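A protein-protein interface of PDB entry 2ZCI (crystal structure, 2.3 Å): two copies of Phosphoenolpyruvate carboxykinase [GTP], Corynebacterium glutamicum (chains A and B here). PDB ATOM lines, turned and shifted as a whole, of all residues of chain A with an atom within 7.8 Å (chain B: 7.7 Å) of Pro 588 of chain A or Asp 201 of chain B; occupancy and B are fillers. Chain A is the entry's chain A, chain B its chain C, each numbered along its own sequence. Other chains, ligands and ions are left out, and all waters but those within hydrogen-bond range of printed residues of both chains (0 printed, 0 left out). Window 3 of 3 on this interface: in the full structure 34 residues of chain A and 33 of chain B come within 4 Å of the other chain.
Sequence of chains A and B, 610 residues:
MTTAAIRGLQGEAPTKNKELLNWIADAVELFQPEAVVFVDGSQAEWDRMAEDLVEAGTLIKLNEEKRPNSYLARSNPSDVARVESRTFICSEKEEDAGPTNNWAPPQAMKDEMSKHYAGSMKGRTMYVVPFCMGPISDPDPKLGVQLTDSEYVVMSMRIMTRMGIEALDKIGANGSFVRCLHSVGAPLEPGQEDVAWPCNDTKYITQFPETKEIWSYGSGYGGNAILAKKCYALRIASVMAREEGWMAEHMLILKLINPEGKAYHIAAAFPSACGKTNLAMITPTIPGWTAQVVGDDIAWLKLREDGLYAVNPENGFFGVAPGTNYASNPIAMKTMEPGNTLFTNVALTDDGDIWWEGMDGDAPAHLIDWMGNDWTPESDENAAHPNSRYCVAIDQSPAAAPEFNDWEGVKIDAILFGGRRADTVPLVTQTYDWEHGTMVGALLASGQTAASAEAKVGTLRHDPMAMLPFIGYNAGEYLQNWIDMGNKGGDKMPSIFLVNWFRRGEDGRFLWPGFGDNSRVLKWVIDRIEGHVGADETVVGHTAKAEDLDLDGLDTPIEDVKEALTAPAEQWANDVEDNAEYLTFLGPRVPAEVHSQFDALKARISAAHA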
ATOM      1  N   GLU A  94      -7.543 -20.480 -26.284  1.00  0.00           N
ATOM      2  CA  GLU A  94      -8.004 -21.004 -25.069  1.00  0.00           C
ATOM      3  C   GLU A  94      -8.927 -22.188 -25.336  1.00  0.00           C
ATOM      4  O   GLU A  94      -9.171 -23.012 -24.468  1.00  0.00           O
ATOM      5  CB  GLU A  94      -8.662 -19.827 -24.296  1.00  0.00           C
ATOM      6  CG  GLU A  94     -10.092 -19.405 -24.650  1.00  0.00           C
ATOM      7  CD  GLU A  94     -11.113 -20.471 -24.261  1.00  0.00           C
ATOM      8  OE1 GLU A  94     -10.902 -21.107 -23.258  1.00  0.00           O
ATOM      9  OE2 GLU A  94     -12.076 -20.717 -24.963  1.00  0.00           O
ATOM     10  N   GLU A  95      -9.435 -22.295 -26.547  1.00  0.00           N
ATOM     11  CA  GLU A  95     -10.408 -23.297 -26.818  1.00  0.00           C
ATOM     12  C   GLU A  95      -9.713 -24.505 -27.432  1.00  0.00           C
ATOM     13  O   GLU A  95     -10.319 -25.577 -27.693  1.00  0.00           O
ATOM     14  CB  GLU A  95     -11.384 -22.690 -27.773  1.00  0.00           C
ATOM     15  CG  GLU A  95     -10.672 -21.627 -28.623  1.00  0.00           C
ATOM     16  CD  GLU A  95     -10.334 -22.293 -29.868  1.00  0.00           C
ATOM     17  OE1 GLU A  95      -9.554 -21.724 -30.689  1.00  0.00           O
ATOM     18  OE2 GLU A  95     -10.899 -23.430 -29.987  1.00  0.00           O
ATOM     19  N   PRO A  99     -12.877 -27.195 -22.483  1.00  0.00           N
ATOM     20  CA  PRO A  99     -13.589 -27.126 -21.197  1.00  0.00           C
ATOM     21  C   PRO A  99     -13.178 -28.085 -20.095  1.00  0.00           C
ATOM     22  O   PRO A  99     -13.730 -28.000 -18.940  1.00  0.00           O
ATOM     23  CB  PRO A  99     -15.060 -27.434 -21.590  1.00  0.00           C
ATOM     24  CG  PRO A  99     -14.923 -28.467 -22.611  1.00  0.00           C
ATOM     25  CD  PRO A  99     -13.757 -27.813 -23.497  1.00  0.00           C
ATOM     26  N   ASN A 474      -8.499 -29.738 -26.862  1.00  0.00           N
ATOM     27  CA  ASN A 474      -9.970 -29.647 -26.720  1.00  0.00           C
ATOM     28  C   ASN A 474     -10.584 -31.082 -26.659  1.00  0.00           C
ATOM     29  O   ASN A 474     -10.415 -31.905 -27.575  1.00  0.00           O
ATOM     30  CB  ASN A 474     -10.603 -28.705 -27.805  1.00  0.00           C
ATOM     31  CG  ASN A 474     -12.080 -28.373 -27.572  1.00  0.00           C
ATOM     32  OD1 ASN A 474     -12.902 -29.230 -27.593  1.00  0.00           O
ATOM     33  ND2 ASN A 474     -12.410 -27.116 -27.448  1.00  0.00           N
ATOM     34  N   GLY A 476     -13.584 -32.302 -27.026  1.00  0.00           N
ATOM     35  CA  GLY A 476     -14.553 -32.702 -28.006  1.00  0.00           C
ATOM     36  C   GLY A 476     -13.764 -32.949 -29.282  1.00  0.00           C
ATOM     37  O   GLY A 476     -14.122 -33.818 -30.085  1.00  0.00           O
ATOM     38  N   GLU A 477     -12.697 -32.184 -29.499  1.00  0.00           N
ATOM     39  CA  GLU A 477     -11.839 -32.466 -30.618  1.00  0.00           C
ATOM     40  C   GLU A 477     -11.059 -33.801 -30.433  1.00  0.00           C
ATOM     41  O   GLU A 477     -10.645 -34.427 -31.403  1.00  0.00           O
ATOM     42  CB  GLU A 477     -10.952 -31.285 -31.007  1.00  0.00           C
ATOM     43  CG  GLU A 477     -10.003 -31.665 -32.187  1.00  0.00           C
ATOM     44  CD  GLU A 477      -8.923 -30.627 -32.473  1.00  0.00           C
ATOM     45  OE1 GLU A 477      -8.895 -29.568 -31.878  1.00  0.00           O
ATOM     46  OE2 GLU A 477      -8.018 -30.932 -33.236  1.00  0.00           O
ATOM     47  N   LEU A 583     -22.457 -34.284 -22.596  1.00  0.00           N
ATOM     48  CA  LEU A 583     -22.071 -34.149 -24.027  1.00  0.00           C
ATOM     49  C   LEU A 583     -22.124 -32.693 -24.447  1.00  0.00           C
ATOM     50  O   LEU A 583     -21.345 -32.240 -25.307  1.00  0.00           O
ATOM     51  CB  LEU A 583     -23.010 -34.952 -24.914  1.00  0.00           C
ATOM     52  CG  LEU A 583     -22.806 -36.412 -24.573  1.00  0.00           C
ATOM     53  CD1 LEU A 583     -23.725 -37.182 -25.468  1.00  0.00           C
ATOM     54  CD2 LEU A 583     -21.301 -36.816 -24.811  1.00  0.00           C
ATOM     55  N   THR A 584     -23.104 -31.962 -23.899  1.00  0.00           N
ATOM     56  CA  THR A 584     -23.170 -30.512 -24.071  1.00  0.00           C
ATOM     57  C   THR A 584     -21.928 -29.849 -23.421  1.00  0.00           C
ATOM     58  O   THR A 584     -21.283 -29.043 -24.026  1.00  0.00           O
ATOM     59  CB  THR A 584     -24.483 -29.953 -23.434  1.00  0.00           C
ATOM     60  OG1 THR A 584     -25.630 -30.443 -24.147  1.00  0.00           O
ATOM     61  CG2 THR A 584     -24.482 -28.396 -23.262  1.00  0.00           C
ATOM     62  N   PHE A 585     -21.632 -30.181 -22.181  1.00  0.00           N
ATOM     63  CA  PHE A 585     -20.496 -29.659 -21.516  1.00  0.00           C
ATOM     64  C   PHE A 585     -19.215 -29.852 -22.362  1.00  0.00           C
ATOM     65  O   PHE A 585     -18.391 -28.975 -22.426  1.00  0.00           O
ATOM     66  CB  PHE A 585     -20.366 -30.323 -20.156  1.00  0.00           C
ATOM     67  CG  PHE A 585     -19.010 -30.151 -19.528  1.00  0.00           C
ATOM     68  CD1 PHE A 585     -18.626 -28.944 -18.990  1.00  0.00           C
ATOM     69  CD2 PHE A 585     -18.133 -31.185 -19.494  1.00  0.00           C
ATOM     70  CE1 PHE A 585     -17.388 -28.807 -18.399  1.00  0.00           C
ATOM     71  CE2 PHE A 585     -16.879 -31.056 -18.947  1.00  0.00           C
ATOM     72  CZ  PHE A 585     -16.495 -29.874 -18.395  1.00  0.00           C
ATOM     73  N   LEU A 586     -19.034 -30.983 -23.017  1.00  0.00           N
ATOM     74  CA  LEU A 586     -17.795 -31.226 -23.707  1.00  0.00           C
ATOM     75  C   LEU A 586     -17.550 -30.293 -24.914  1.00  0.00           C
ATOM     76  O   LEU A 586     -16.408 -30.186 -25.428  1.00  0.00           O
ATOM     77  CB  LEU A 586     -17.669 -32.726 -24.049  1.00  0.00           C
ATOM     78  CG  LEU A 586     -17.267 -33.844 -23.059  1.00  0.00           C
ATOM     79  CD1 LEU A 586     -17.263 -35.171 -23.757  1.00  0.00           C
ATOM     80  CD2 LEU A 586     -15.891 -33.492 -22.482  1.00  0.00           C
ATOM     81  N   GLY A 587     -18.620 -29.641 -25.386  1.00  0.00           N
ATOM     82  CA  GLY A 587     -18.535 -28.402 -26.227  1.00  0.00           C
ATOM     83  C   GLY A 587     -18.905 -28.576 -27.707  1.00  0.00           C
ATOM     84  O   GLY A 587     -19.340 -29.696 -28.119  1.00  0.00           O
ATOM     85  N   PRO A 588     -18.710 -27.494 -28.528  1.00  0.00           N
ATOM     86  CA  PRO A 588     -18.969 -27.522 -29.975  1.00  0.00           C
ATOM     87  C   PRO A 588     -18.042 -28.331 -30.883  1.00  0.00           C
ATOM     88  O   PRO A 588     -18.260 -28.248 -32.049  1.00  0.00           O
ATOM     89  CB  PRO A 588     -18.885 -26.038 -30.404  1.00  0.00           C
ATOM     90  CG  PRO A 588     -17.912 -25.403 -29.331  1.00  0.00           C
ATOM     91  CD  PRO A 588     -18.280 -26.134 -28.066  1.00  0.00           C
ATOM     92  N   ARG A 589     -17.008 -29.057 -30.389  1.00  0.00           N
ATOM     93  CA  ARG A 589     -16.220 -29.960 -31.233  1.00  0.00           C
ATOM     94  C   ARG A 589     -16.575 -31.409 -31.025  1.00  0.00           C
ATOM     95  O   ARG A 589     -16.091 -32.282 -31.812  1.00  0.00           O
ATOM     96  CB  ARG A 589     -14.755 -29.750 -30.985  1.00  0.00           C
ATOM     97  CG  ARG A 589     -14.366 -28.352 -31.198  1.00  0.00           C
ATOM     98  CD  ARG A 589     -12.880 -28.265 -31.392  1.00  0.00           C
ATOM     99  NE  ARG A 589     -12.541 -26.938 -31.870  1.00  0.00           N
ATOM    100  CZ  ARG A 589     -11.696 -26.121 -31.274  1.00  0.00           C
ATOM    101  NH1 ARG A 589     -11.036 -26.513 -30.216  1.00  0.00           N
ATOM    102  NH2 ARG A 589     -11.484 -24.925 -31.758  1.00  0.00           N
ATOM    103  N   VAL A 590     -17.361 -31.699 -29.979  1.00  0.00           N
ATOM    104  CA  VAL A 590     -18.096 -32.981 -29.925  1.00  0.00           C
ATOM    105  C   VAL A 590     -18.683 -33.400 -31.280  1.00  0.00           C
ATOM    106  O   VAL A 590     -19.573 -32.735 -31.876  1.00  0.00           O
ATOM    107  CB  VAL A 590     -19.165 -33.124 -28.799  1.00  0.00           C
ATOM    108  CG1 VAL A 590     -19.721 -34.598 -28.759  1.00  0.00           C
ATOM    109  CG2 VAL A 590     -18.525 -32.748 -27.447  1.00  0.00           C
ATOM    110  N   PRO A 591     -18.166 -34.527 -31.780  1.00  0.00           N
ATOM    111  CA  PRO A 591     -18.655 -34.841 -33.106  1.00  0.00           C
ATOM    112  C   PRO A 591     -20.205 -35.130 -33.127  1.00  0.00           C
ATOM    113  O   PRO A 591     -20.780 -35.639 -32.142  1.00  0.00           O
ATOM    114  CB  PRO A 591     -17.835 -36.105 -33.484  1.00  0.00           C
ATOM    115  CG  PRO A 591     -16.517 -36.030 -32.606  1.00  0.00           C
ATOM    116  CD  PRO A 591     -17.080 -35.420 -31.288  1.00  0.00           C
ATOM    117  N   ALA A 592     -20.836 -34.813 -34.261  1.00  0.00           N
ATOM    118  CA  ALA A 592     -22.207 -35.128 -34.596  1.00  0.00           C
ATOM    119  C   ALA A 592     -22.384 -36.619 -34.510  1.00  0.00           C
ATOM    120  O   ALA A 592     -23.456 -37.118 -34.205  1.00  0.00           O
ATOM    121  CB  ALA A 592     -22.490 -34.696 -36.113  1.00  0.00           C
ATOM    122  N   HIS A 595     -23.241 -37.303 -30.795  1.00  0.00           N
ATOM    123  CA  HIS A 595     -24.623 -36.904 -30.589  1.00  0.00           C
ATOM    124  C   HIS A 595     -25.556 -37.856 -31.269  1.00  0.00           C
ATOM    125  O   HIS A 595     -26.542 -38.261 -30.666  1.00  0.00           O
ATOM    126  CB  HIS A 595     -24.871 -35.461 -31.108  1.00  0.00           C
ATOM    127  CG  HIS A 595     -24.047 -34.419 -30.411  1.00  0.00           C
ATOM    128  ND1 HIS A 595     -24.184 -34.134 -29.062  1.00  0.00           N
ATOM    129  CD2 HIS A 595     -23.106 -33.566 -30.878  1.00  0.00           C
ATOM    130  CE1 HIS A 595     -23.320 -33.182 -28.724  1.00  0.00           C
ATOM    131  NE2 HIS A 595     -22.670 -32.805 -29.812  1.00  0.00           N
ATOM    132  N   ASN B  76     -29.334 -20.397 -24.530  1.00  0.00           N
ATOM    133  CA  ASN B  76     -28.591 -21.336 -25.282  1.00  0.00           C
ATOM    134  C   ASN B  76     -28.089 -22.492 -24.429  1.00  0.00           C
ATOM    135  O   ASN B  76     -27.474 -22.229 -23.425  1.00  0.00           O
ATOM    136  CB  ASN B  76     -27.366 -20.633 -25.799  1.00  0.00           C
ATOM    137  CG  ASN B  76     -27.054 -21.076 -27.089  1.00  0.00           C
ATOM    138  OD1 ASN B  76     -26.609 -22.166 -27.238  1.00  0.00           O
ATOM    139  ND2 ASN B  76     -27.412 -20.306 -28.082  1.00  0.00           N
ATOM    140  N   SER B  78     -25.663 -24.351 -24.330  1.00  0.00           N
ATOM    141  CA  SER B  78     -24.297 -24.257 -23.819  1.00  0.00           C
ATOM    142  C   SER B  78     -23.998 -22.830 -23.366  1.00  0.00           C
ATOM    143  O   SER B  78     -23.304 -22.094 -24.088  1.00  0.00           O
ATOM    144  CB  SER B  78     -23.311 -24.686 -24.869  1.00  0.00           C
ATOM    145  OG  SER B  78     -23.521 -23.907 -25.998  1.00  0.00           O
ATOM    146  N   VAL B  83     -19.202 -22.623 -15.589  1.00  0.00           N
ATOM    147  CA  VAL B  83     -17.819 -22.349 -16.222  1.00  0.00           C
ATOM    148  C   VAL B  83     -16.625 -22.129 -15.277  1.00  0.00           C
ATOM    149  O   VAL B  83     -15.901 -21.185 -15.484  1.00  0.00           O
ATOM    150  CB  VAL B  83     -17.688 -21.261 -17.397  1.00  0.00           C
ATOM    151  CG1 VAL B  83     -18.451 -21.615 -18.611  1.00  0.00           C
ATOM    152  CG2 VAL B  83     -18.036 -19.868 -17.021  1.00  0.00           C
ATOM    153  N   ARG B  86     -12.940 -21.626 -16.447  1.00  0.00           N
ATOM    154  CA  ARG B  86     -12.683 -20.271 -16.963  1.00  0.00           C
ATOM    155  C   ARG B  86     -13.116 -19.199 -16.003  1.00  0.00           C
ATOM    156  O   ARG B  86     -13.530 -18.125 -16.415  1.00  0.00           O
ATOM    157  CB  ARG B  86     -13.339 -20.079 -18.350  1.00  0.00           C
ATOM    158  CG  ARG B  86     -12.798 -21.008 -19.473  1.00  0.00           C
ATOM    159  CD  ARG B  86     -11.354 -20.655 -19.943  1.00  0.00           C
ATOM    160  NE  ARG B  86     -10.843 -21.651 -20.845  1.00  0.00           N
ATOM    161  CZ  ARG B  86     -10.142 -22.761 -20.500  1.00  0.00           C
ATOM    162  NH1 ARG B  86      -9.841 -23.057 -19.219  1.00  0.00           N
ATOM    163  NH2 ARG B  86      -9.754 -23.623 -21.452  1.00  0.00           N
ATOM    164  N   VAL B 184     -21.862  -9.970 -23.752  1.00  0.00           N
ATOM    165  CA  VAL B 184     -22.243 -11.345 -24.083  1.00  0.00           C
ATOM    166  C   VAL B 184     -21.389 -11.869 -25.268  1.00  0.00           C
ATOM    167  O   VAL B 184     -21.524 -13.040 -25.593  1.00  0.00           O
ATOM    168  CB  VAL B 184     -23.793 -11.487 -24.427  1.00  0.00           C
ATOM    169  CG1 VAL B 184     -24.682 -11.272 -23.129  1.00  0.00           C
ATOM    170  CG2 VAL B 184     -24.242 -10.528 -25.649  1.00  0.00           C
ATOM    171  N   GLY B 185     -20.553 -11.003 -25.898  1.00  0.00           N
ATOM    172  CA  GLY B 185     -19.613 -11.356 -26.989  1.00  0.00           C
ATOM    173  C   GLY B 185     -20.295 -11.762 -28.293  1.00  0.00           C
ATOM    174  O   GLY B 185     -20.022 -12.830 -28.875  1.00  0.00           O
ATOM    175  N   CYS B 199     -24.443 -14.829 -27.140  1.00  0.00           N
ATOM    176  CA  CYS B 199     -23.348 -15.522 -26.353  1.00  0.00           C
ATOM    177  C   CYS B 199     -22.077 -15.958 -27.173  1.00  0.00           C
ATOM    178  O   CYS B 199     -22.067 -15.872 -28.412  1.00  0.00           O
ATOM    179  CB  CYS B 199     -23.880 -16.686 -25.447  1.00  0.00           C
ATOM    180  SG  CYS B 199     -24.551 -18.189 -26.253  1.00  0.00           S
ATOM    181  N   ASN B 200     -21.004 -16.388 -26.498  1.00  0.00           N
ATOM    182  CA  ASN B 200     -19.795 -16.759 -27.186  1.00  0.00           C
ATOM    183  C   ASN B 200     -19.335 -18.121 -26.741  1.00  0.00           C
ATOM    184  O   ASN B 200     -19.461 -18.441 -25.541  1.00  0.00           O
ATOM    185  CB  ASN B 200     -18.642 -15.756 -26.936  1.00  0.00           C
ATOM    186  CG  ASN B 200     -17.614 -15.731 -28.118  1.00  0.00           C
ATOM    187  OD1 ASN B 200     -16.936 -16.713 -28.407  1.00  0.00           O
ATOM    188  ND2 ASN B 200     -17.518 -14.615 -28.783  1.00  0.00           N
ATOM    189  N   ASP B 201     -18.783 -18.896 -27.680  1.00  0.00           N
ATOM    190  CA  ASP B 201     -18.096 -20.184 -27.378  1.00  0.00           C
ATOM    191  C   ASP B 201     -16.838 -20.016 -26.448  1.00  0.00           C
ATOM    192  O   ASP B 201     -16.453 -20.958 -25.705  1.00  0.00           O
ATOM    193  CB  ASP B 201     -17.756 -20.971 -28.664  1.00  0.00           C
ATOM    194  CG  ASP B 201     -19.007 -21.586 -29.337  1.00  0.00           C
ATOM    195  OD1 ASP B 201     -18.892 -21.935 -30.511  1.00  0.00           O
ATOM    196  OD2 ASP B 201     -20.094 -21.756 -28.709  1.00  0.00           O
ATOM    197  N   THR B 202     -16.247 -18.814 -26.458  1.00  0.00           N
ATOM    198  CA  THR B 202     -15.275 -18.409 -25.467  1.00  0.00           C
ATOM    199  C   THR B 202     -15.951 -17.714 -24.281  1.00  0.00           C
ATOM    200  O   THR B 202     -16.613 -16.729 -24.429  1.00  0.00           O
ATOM    201  CB  THR B 202     -14.186 -17.561 -26.092  1.00  0.00           C
ATOM    202  OG1 THR B 202     -13.450 -18.315 -27.079  1.00  0.00           O
ATOM    203  CG2 THR B 202     -13.216 -17.142 -25.009  1.00  0.00           C
ATOM    204  N   LYS B 203     -15.801 -18.230 -23.092  1.00  0.00           N
ATOM    205  CA  LYS B 203     -16.422 -17.628 -21.938  1.00  0.00           C
ATOM    206  C   LYS B 203     -15.385 -17.449 -20.854  1.00  0.00           C
ATOM    207  O   LYS B 203     -14.732 -18.380 -20.522  1.00  0.00           O
ATOM    208  CB  LYS B 203     -17.646 -18.473 -21.444  1.00  0.00           C
ATOM    209  CG  LYS B 203     -18.699 -18.839 -22.513  1.00  0.00           C
ATOM    210  CD  LYS B 203     -19.699 -19.945 -22.054  1.00  0.00           C
ATOM    211  CE  LYS B 203     -20.025 -20.955 -23.199  1.00  0.00           C
ATOM    212  NZ  LYS B 203     -20.791 -20.197 -24.265  1.00  0.00           N
ATOM    213  N   TYR B 204     -15.252 -16.250 -20.310  1.00  0.00           N
ATOM    214  CA  TYR B 204     -14.345 -15.892 -19.230  1.00  0.00           C
ATOM    215  C   TYR B 204     -15.064 -15.173 -18.030  1.00  0.00           C
ATOM    216  O   TYR B 204     -15.866 -14.293 -18.245  1.00  0.00           O
ATOM    217  CB  TYR B 204     -13.343 -14.907 -19.759  1.00  0.00           C
ATOM    218  CG  TYR B 204     -12.306 -15.444 -20.683  1.00  0.00           C
ATOM    219  CD1 TYR B 204     -12.131 -14.866 -21.952  1.00  0.00           C
ATOM    220  CD2 TYR B 204     -11.447 -16.501 -20.286  1.00  0.00           C
ATOM    221  CE1 TYR B 204     -11.179 -15.344 -22.838  1.00  0.00           C
ATOM    222  CE2 TYR B 204     -10.528 -17.006 -21.133  1.00  0.00           C
ATOM    223  CZ  TYR B 204     -10.362 -16.403 -22.417  1.00  0.00           C
ATOM    224  OH  TYR B 204      -9.369 -16.856 -23.289  1.00  0.00           O
ATOM    225  N   TYR B 217     -17.146 -12.269 -19.868  1.00  0.00           N
ATOM    226  CA  TYR B 217     -17.254 -12.343 -21.331  1.00  0.00           C
ATOM    227  C   TYR B 217     -17.941 -13.664 -21.827  1.00  0.00           C
ATOM    228  O   TYR B 217     -17.649 -14.768 -21.342  1.00  0.00           O
ATOM    229  CB  TYR B 217     -15.914 -12.050 -22.014  1.00  0.00           C
ATOM    230  CG  TYR B 217     -15.963 -12.235 -23.484  1.00  0.00           C
ATOM    231  CD1 TYR B 217     -15.706 -13.503 -24.053  1.00  0.00           C
ATOM    232  CD2 TYR B 217     -16.315 -11.156 -24.348  1.00  0.00           C
ATOM    233  CE1 TYR B 217     -15.762 -13.685 -25.454  1.00  0.00           C
ATOM    234  CE2 TYR B 217     -16.378 -11.320 -25.745  1.00  0.00           C
ATOM    235  CZ  TYR B 217     -16.107 -12.584 -26.295  1.00  0.00           C
ATOM    236  OH  TYR B 217     -16.179 -12.756 -27.673  1.00  0.00           O
ATOM    237  N   GLY B 218     -18.915 -13.505 -22.733  1.00  0.00           N
ATOM    238  CA  GLY B 218     -19.428 -14.639 -23.533  1.00  0.00           C
ATOM    239  C   GLY B 218     -20.634 -15.355 -22.971  1.00  0.00           C
ATOM    240  O   GLY B 218     -21.232 -16.249 -23.601  1.00  0.00           O
ATOM    241  N   SER B 219     -21.000 -14.923 -21.773  1.00  0.00           N
ATOM    242  CA  SER B 219     -22.100 -15.568 -21.031  1.00  0.00           C
ATOM    243  C   SER B 219     -23.186 -14.605 -20.576  1.00  0.00           C
ATOM    244  O   SER B 219     -22.908 -13.664 -19.835  1.00  0.00           O
ATOM    245  CB  SER B 219     -21.564 -16.330 -19.862  1.00  0.00           C
ATOM    246  OG  SER B 219     -22.641 -16.903 -19.196  1.00  0.00           O
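The backbone NH (N) of Thr 202 of chain B lies within hydrogen-bond range of the side-chain amide oxygen (OD1) of Asn 200 of chain B (2.9 Å). The backbone carbonyl oxygen (O) of Tyr 204 of chain B lies within hydrogen-bond range of the backbone NH (N) of Tyr 217 of chain B (2.9 Å).
Of the printed residues of chain B, Glu 94 of chain A touches Arg 86, Thr 202 and Tyr 204. Glu 477 of chain A touches none of the printed residues of chain B. Leu 583 of chain A touches none of the printed residues of chain B. Pro 588 of chain A touches just one residue of chain B: Asp 201. Of the printed residues of chain A, Arg 86 of chain B touches Glu 94. Asp 201 of chain B touches just one residue of chain A: Pro 588. Of the printed residues of chain A, Tyr 204 of chain B touches Glu 94. The nearest printed residue of chain A that does not touch Thr 202 of chain B is Glu 95 of chain A (4.6 Å).
The side-chain carboxylate of Glu 94 of chain A lies within salt-bridge range of the guanidinium group of Arg 86 of chain B (2.5 Å). The side-chain carboxylate (OE2) of Glu 94 of chain A is in hydrogen-bond range of the side-chain hydroxyl (OG1) of Thr 202 of chain B (3.5 Å).
Tyr 204 of chain B touches Glu 94 of chain A (OH to CG, 3.0 Å). Pro 588 of chain A touches Asp 201 of chain B (CG to OD1, 3.8 Å).
No position is printed for both chains.
Of the 17 printed residues of chain A, 2 touch a printed residue of chain B. Hydrophobic or aromatic side chains of chain A that line the printed part of chain B: Pro 588. Hydrophobic or aromatic side chains of chain B within 4 Å of the printed part of chain A: Tyr 204. Among the printed residues, 4 pairs touch across the chains.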
